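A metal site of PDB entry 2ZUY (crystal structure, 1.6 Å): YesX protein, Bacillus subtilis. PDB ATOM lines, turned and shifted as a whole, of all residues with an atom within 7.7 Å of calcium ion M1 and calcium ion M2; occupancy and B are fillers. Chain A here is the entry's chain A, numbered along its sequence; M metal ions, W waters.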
ATOM      1  N   LYS A   4      24.415 -20.905  -5.990  1.00  0.00           N
ATOM      2  CA  LYS A   4      23.057 -21.403  -5.767  1.00  0.00           C
ATOM      3  C   LYS A   4      22.099 -20.694  -6.724  1.00  0.00           C
ATOM      4  O   LYS A   4      22.273 -19.511  -7.011  1.00  0.00           O
ATOM      5  CB  LYS A   4      22.610 -21.114  -4.338  1.00  0.00           C
ATOM      6  CG  LYS A   4      23.328 -21.890  -3.248  1.00  0.00           C
ATOM      7  CD  LYS A   4      22.766 -21.539  -1.872  1.00  0.00           C
ATOM      8  CE  LYS A   4      23.498 -20.368  -1.236  1.00  0.00           C
ATOM      9  NZ  LYS A   4      24.760 -20.793  -0.579  1.00  0.00           N
ATOM     10  N   ARG A   6      18.595 -19.034  -7.328  1.00  0.00           N
ATOM     11  CA  ARG A   6      17.523 -18.403  -6.556  1.00  0.00           C
ATOM     12  C   ARG A   6      16.187 -18.485  -7.279  1.00  0.00           C
ATOM     13  O   ARG A   6      16.106 -18.293  -8.491  1.00  0.00           O
ATOM     14  CB  ARG A   6      17.836 -16.924  -6.309  1.00  0.00           C
ATOM     15  CG  ARG A   6      18.937 -16.710  -5.303  1.00  0.00           C
ATOM     16  CD  ARG A   6      19.084 -15.234  -4.947  1.00  0.00           C
ATOM     17  NE  ARG A   6      20.071 -15.067  -3.885  1.00  0.00           N
ATOM     18  CZ  ARG A   6      20.030 -14.128  -2.942  1.00  0.00           C
ATOM     19  NH1 ARG A   6      19.045 -13.239  -2.904  1.00  0.00           N
ATOM     20  NH2 ARG A   6      20.986 -14.104  -2.013  1.00  0.00           N
ATOM     21  N   TYR A 278      16.617 -13.863   0.972  1.00  0.00           N
ATOM     22  CA  TYR A 278      16.901 -15.260   0.685  1.00  0.00           C
ATOM     23  C   TYR A 278      17.919 -15.760   1.705  1.00  0.00           C
ATOM     24  O   TYR A 278      19.112 -15.890   1.419  1.00  0.00           O
ATOM     25  CB  TYR A 278      17.422 -15.440  -0.754  1.00  0.00           C
ATOM     26  CG  TYR A 278      16.344 -15.315  -1.807  1.00  0.00           C
ATOM     27  CD1 TYR A 278      16.093 -16.352  -2.707  1.00  0.00           C
ATOM     28  CD2 TYR A 278      15.558 -14.153  -1.903  1.00  0.00           C
ATOM     29  CE1 TYR A 278      15.103 -16.243  -3.686  1.00  0.00           C
ATOM     30  CE2 TYR A 278      14.564 -14.032  -2.876  1.00  0.00           C
ATOM     31  CZ  TYR A 278      14.339 -15.085  -3.759  1.00  0.00           C
ATOM     32  OH  TYR A 278      13.367 -14.969  -4.707  1.00  0.00           O
ATOM     33  N   LEU A 279      17.431 -16.047   2.905  1.00  0.00           N
ATOM     34  CA  LEU A 279      18.279 -16.426   4.037  1.00  0.00           C
ATOM     35  C   LEU A 279      18.978 -17.771   3.830  1.00  0.00           C
ATOM     36  O   LEU A 279      20.035 -18.014   4.414  1.00  0.00           O
ATOM     37  CB  LEU A 279      17.477 -16.374   5.346  1.00  0.00           C
ATOM     38  CG  LEU A 279      16.843 -15.015   5.665  1.00  0.00           C
ATOM     39  CD1 LEU A 279      15.875 -15.113   6.842  1.00  0.00           C
ATOM     40  CD2 LEU A 279      17.897 -13.946   5.930  1.00  0.00           C
ATOM     41  N   ALA A 335      21.132  -8.070   0.988  1.00  0.00           N
ATOM     42  CA  ALA A 335      22.125  -8.493  -0.003  1.00  0.00           C
ATOM     43  C   ALA A 335      23.008  -9.576   0.577  1.00  0.00           C
ATOM     44  O   ALA A 335      23.184  -9.654   1.800  1.00  0.00           O
ATOM     45  CB  ALA A 335      22.981  -7.316  -0.437  1.00  0.00           C
ATOM     46  N   ASP A 336      23.582 -10.389  -0.311  1.00  0.00           N
ATOM     47  CA  ASP A 336      24.667 -11.279   0.098  1.00  0.00           C
ATOM     48  C   ASP A 336      25.944 -10.449   0.192  1.00  0.00           C
ATOM     49  O   ASP A 336      26.552 -10.093  -0.834  1.00  0.00           O
ATOM     50  CB  ASP A 336      24.827 -12.443  -0.878  1.00  0.00           C
ATOM     51  CG  ASP A 336      26.034 -13.306  -0.561  1.00  0.00           C
ATOM     52  OD1 ASP A 336      26.577 -13.197   0.568  1.00  0.00           O
ATOM     53  OD2 ASP A 336      26.444 -14.093  -1.438  1.00  0.00           O
ATOM     54  N   VAL A 337      26.336 -10.139   1.424  1.00  0.00           N
ATOM     55  CA  VAL A 337      27.464  -9.232   1.663  1.00  0.00           C
ATOM     56  C   VAL A 337      28.763  -9.949   2.039  1.00  0.00           C
ATOM     57  O   VAL A 337      29.836  -9.336   2.065  1.00  0.00           O
ATOM     58  CB  VAL A 337      27.129  -8.139   2.713  1.00  0.00           C
ATOM     59  CG1 VAL A 337      25.995  -7.276   2.227  1.00  0.00           C
ATOM     60  CG2 VAL A 337      26.785  -8.772   4.073  1.00  0.00           C
ATOM     61  N   ASP A 338      28.672 -11.243   2.339  1.00  0.00           N
ATOM     62  CA  ASP A 338      29.839 -11.998   2.804  1.00  0.00           C
ATOM     63  C   ASP A 338      30.243 -13.147   1.874  1.00  0.00           C
ATOM     64  O   ASP A 338      31.157 -13.910   2.196  1.00  0.00           O
ATOM     65  CB  ASP A 338      29.652 -12.466   4.266  1.00  0.00           C
ATOM     66  CG  ASP A 338      28.454 -13.386   4.456  1.00  0.00           C
ATOM     67  OD1 ASP A 338      27.846 -13.823   3.453  1.00  0.00           O
ATOM     68  OD2 ASP A 338      28.119 -13.673   5.621  1.00  0.00           O
ATOM     69  N   GLY A 339      29.571 -13.265   0.736  1.00  0.00           N
ATOM     70  CA  GLY A 339      29.935 -14.223  -0.309  1.00  0.00           C
ATOM     71  C   GLY A 339      29.491 -15.662  -0.126  1.00  0.00           C
ATOM     72  O   GLY A 339      29.959 -16.548  -0.856  1.00  0.00           O
ATOM     73  N   ASP A 340      28.603 -15.935   0.835  1.00  0.00           N
ATOM     74  CA  ASP A 340      28.132 -17.302   1.056  1.00  0.00           C
ATOM     75  C   ASP A 340      26.860 -17.663   0.284  1.00  0.00           C
ATOM     76  O   ASP A 340      26.299 -18.750   0.470  1.00  0.00           O
ATOM     77  CB  ASP A 340      27.988 -17.607   2.558  1.00  0.00           C
ATOM     78  CG  ASP A 340      26.938 -16.751   3.241  1.00  0.00           C
ATOM     79  OD1 ASP A 340      26.127 -16.099   2.538  1.00  0.00           O
ATOM     80  OD2 ASP A 340      26.919 -16.716   4.496  1.00  0.00           O
ATOM     81  N   GLY A 341      26.395 -16.741  -0.556  1.00  0.00           N
ATOM     82  CA  GLY A 341      25.215 -16.958  -1.407  1.00  0.00           C
ATOM     83  C   GLY A 341      23.890 -16.630  -0.719  1.00  0.00           C
ATOM     84  O   GLY A 341      22.841 -16.567  -1.371  1.00  0.00           O
ATOM     85  N   LYS A 342      23.953 -16.411   0.581  1.00  0.00           N
ATOM     86  CA  LYS A 342      22.763 -16.168   1.396  1.00  0.00           C
ATOM     87  C   LYS A 342      22.645 -14.685   1.715  1.00  0.00           C
ATOM     88  O   LYS A 342      23.647 -13.995   1.847  1.00  0.00           O
ATOM     89  CB  LYS A 342      22.837 -17.001   2.679  1.00  0.00           C
ATOM     90  CG  LYS A 342      23.025 -18.501   2.425  1.00  0.00           C
ATOM     91  CD  LYS A 342      23.257 -19.278   3.697  1.00  0.00           C
ATOM     92  CE  LYS A 342      23.535 -20.741   3.388  1.00  0.00           C
ATOM     93  NZ  LYS A 342      23.750 -21.534   4.632  1.00  0.00           N
ATOM     94  N   ASP A 343      21.412 -14.193   1.834  1.00  0.00           N
ATOM     95  CA  ASP A 343      21.209 -12.774   2.135  1.00  0.00           C
ATOM     96  C   ASP A 343      21.405 -12.449   3.595  1.00  0.00           C
ATOM     97  O   ASP A 343      20.915 -13.168   4.482  1.00  0.00           O
ATOM     98  CB  ASP A 343      19.813 -12.298   1.731  1.00  0.00           C
ATOM     99  CG  ASP A 343      19.674 -12.119   0.237  1.00  0.00           C
ATOM    100  OD1 ASP A 343      20.669 -11.801  -0.436  1.00  0.00           O
ATOM    101  OD2 ASP A 343      18.534 -12.285  -0.258  1.00  0.00           O
ATOM    102  N   GLU A 344      22.089 -11.339   3.827  1.00  0.00           N
ATOM    103  CA  GLU A 344      22.136 -10.696   5.143  1.00  0.00           C
ATOM    104  C   GLU A 344      21.210  -9.479   5.133  1.00  0.00           C
ATOM    105  O   GLU A 344      20.814  -8.991   4.064  1.00  0.00           O
ATOM    106  CB  GLU A 344      23.573 -10.282   5.491  1.00  0.00           C
ATOM    107  CG  GLU A 344      24.498 -11.458   5.850  1.00  0.00           C
ATOM    108  CD  GLU A 344      24.916 -12.289   4.653  1.00  0.00           C
ATOM    109  OE1 GLU A 344      24.945 -13.534   4.773  1.00  0.00           O
ATOM    110  OE2 GLU A 344      25.245 -11.723   3.579  1.00  0.00           O
ATOM    111  N   VAL A 352      22.547  -7.922  10.348  1.00  0.00           N
ATOM    112  CA  VAL A 352      22.183  -9.215  10.897  1.00  0.00           C
ATOM    113  C   VAL A 352      22.528 -10.311   9.875  1.00  0.00           C
ATOM    114  O   VAL A 352      22.231 -10.173   8.678  1.00  0.00           O
ATOM    115  CB  VAL A 352      20.683  -9.254  11.269  1.00  0.00           C
ATOM    116  CG1 VAL A 352      20.257 -10.652  11.717  1.00  0.00           C
ATOM    117  CG2 VAL A 352      20.385  -8.233  12.368  1.00  0.00           C
ATOM    118  N   ASP A 353      23.175 -11.376  10.338  1.00  0.00           N
ATOM    119  CA  ASP A 353      23.603 -12.460   9.461  1.00  0.00           C
ATOM    120  C   ASP A 353      22.391 -13.271   8.969  1.00  0.00           C
ATOM    121  O   ASP A 353      21.280 -13.129   9.492  1.00  0.00           O
ATOM    122  CB  ASP A 353      24.616 -13.357  10.192  1.00  0.00           C
ATOM    123  CG  ASP A 353      25.595 -14.049   9.236  1.00  0.00           C
ATOM    124  OD1 ASP A 353      25.474 -13.893   7.999  1.00  0.00           O
ATOM    125  OD2 ASP A 353      26.499 -14.729   9.740  1.00  0.00           O
ATOM    126  N   HIS A 354      22.604 -14.107   7.954  1.00  0.00           N
ATOM    127  CA  HIS A 354      21.520 -14.897   7.339  1.00  0.00           C
ATOM    128  C   HIS A 354      20.819 -15.835   8.329  1.00  0.00           C
ATOM    129  O   HIS A 354      19.699 -16.274   8.073  1.00  0.00           O
ATOM    130  CB  HIS A 354      22.058 -15.723   6.170  1.00  0.00           C
ATOM    131  CG  HIS A 354      22.970 -16.824   6.584  1.00  0.00           C
ATOM    132  ND1 HIS A 354      24.340 -16.681   6.650  1.00  0.00           N
ATOM    133  CD2 HIS A 354      22.713 -18.092   6.986  1.00  0.00           C
ATOM    134  CE1 HIS A 354      24.880 -17.814   7.073  1.00  0.00           C
ATOM    135  NE2 HIS A 354      23.916 -18.682   7.281  1.00  0.00           N
ATOM    136  N   ASP A 355      21.495 -16.145   9.434  1.00  0.00           N
ATOM    137  CA  ASP A 355      21.000 -17.073  10.438  1.00  0.00           C
ATOM    138  C   ASP A 355      20.445 -16.362  11.685  1.00  0.00           C
ATOM    139  O   ASP A 355      20.165 -17.004  12.699  1.00  0.00           O
ATOM    140  CB  ASP A 355      22.097 -18.081  10.824  1.00  0.00           C
ATOM    141  CG  ASP A 355      23.295 -17.426  11.486  1.00  0.00           C
ATOM    142  OD1 ASP A 355      23.339 -16.184  11.578  1.00  0.00           O
ATOM    143  OD2 ASP A 355      24.212 -18.171  11.932  1.00  0.00           O
ATOM    144  N   THR A 357      21.976 -14.235  13.624  1.00  0.00           N
ATOM    145  CA  THR A 357      23.028 -13.802  14.551  1.00  0.00           C
ATOM    146  C   THR A 357      23.494 -12.408  14.136  1.00  0.00           C
ATOM    147  O   THR A 357      23.272 -11.990  13.003  1.00  0.00           O
ATOM    148  CB  THR A 357      24.226 -14.764  14.574  1.00  0.00           C
ATOM    149  OG1 THR A 357      24.840 -14.819  13.281  1.00  0.00           O
ATOM    150  CG2 THR A 357      23.795 -16.174  15.012  1.00  0.00           C
ATOM    151  N   LEU A 359      25.815  -9.742  12.672  1.00  0.00           N
ATOM    152  CA  LEU A 359      26.944  -9.721  11.749  1.00  0.00           C
ATOM    153  C   LEU A 359      27.958  -8.693  12.234  1.00  0.00           C
ATOM    154  O   LEU A 359      29.107  -9.032  12.543  1.00  0.00           O
ATOM    155  CB  LEU A 359      26.497  -9.432  10.307  1.00  0.00           C
ATOM    156  CG  LEU A 359      27.518  -9.691   9.186  1.00  0.00           C
ATOM    157  CD1 LEU A 359      27.834 -11.186   9.010  1.00  0.00           C
ATOM    158  CD2 LEU A 359      27.037  -9.106   7.864  1.00  0.00           C
HETATM  159 CA    CA M   1      25.752 -13.905   2.582  1.00  0.00          CA
HETATM  160 CA    CA M   2      26.200 -15.061   5.993  1.00  0.00          CA
HETATM  161  O   HOH W   1      27.577 -16.136   7.574  1.00  0.00           O
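Calcium ion M2 is bound by OE1 of Glu 344 (2.3 Å), OD2 of Asp 340 (2.3 Å), water W1 (2.4 Å), OD2 of Asp 338 (2.4 Å), OD1 of Asp 353 (2.4 Å) and ND1 of His 354 (2.6 Å). Calcium ion M2 has six donor atoms within binding distance.
Calcium ion M1 is bound by OD1 of Asp 340 (2.2 Å), O of Lys 342 (2.2 Å), OD1 of Asp 338 (2.3 Å), OD1 of Asp 336 (2.3 Å), OE1 of Glu 344 (2.4 Å) and OE2 of Glu 344 (2.5 Å).
Residues that only touch calcium ion M1: Val 337 (3.98 Å). Of the 20 residues printed, 6 come within 4 Å of calcium ion M1. Along chain A the residues within 4 Å of calcium ion M1 span positions 336 to 344. The nearest printed residue that does not touch calcium ion M1 is Gly 341 (4.3 Å).
O of Asp 340 is in hydrogen-bond range of NZ of Lys 4. OD2 of Asp 336 lies within hydrogen-bond range of N of Gly 341 (2.8 Å). N of Gly 339 sits close to OD1 of Asp 336, at 3.0 Å. The side-chain carboxylate of Asp 343 lies within hydrogen-bond range of the backbone NH of Asp 336, at 3.2 Å. The backbone NH of Val 337 lies close to the side-chain carboxylate of Glu 344 (2.9 Å). The backbone NH of Glu 344 sits at hydrogen-bond distance from the backbone carbonyl oxygen of Ala 335 (2.9 Å).
Five residues have an atom within 4 Å of calcium ion M2: Asp 338, Asp 340, Glu 344, Asp 353 and His 354.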
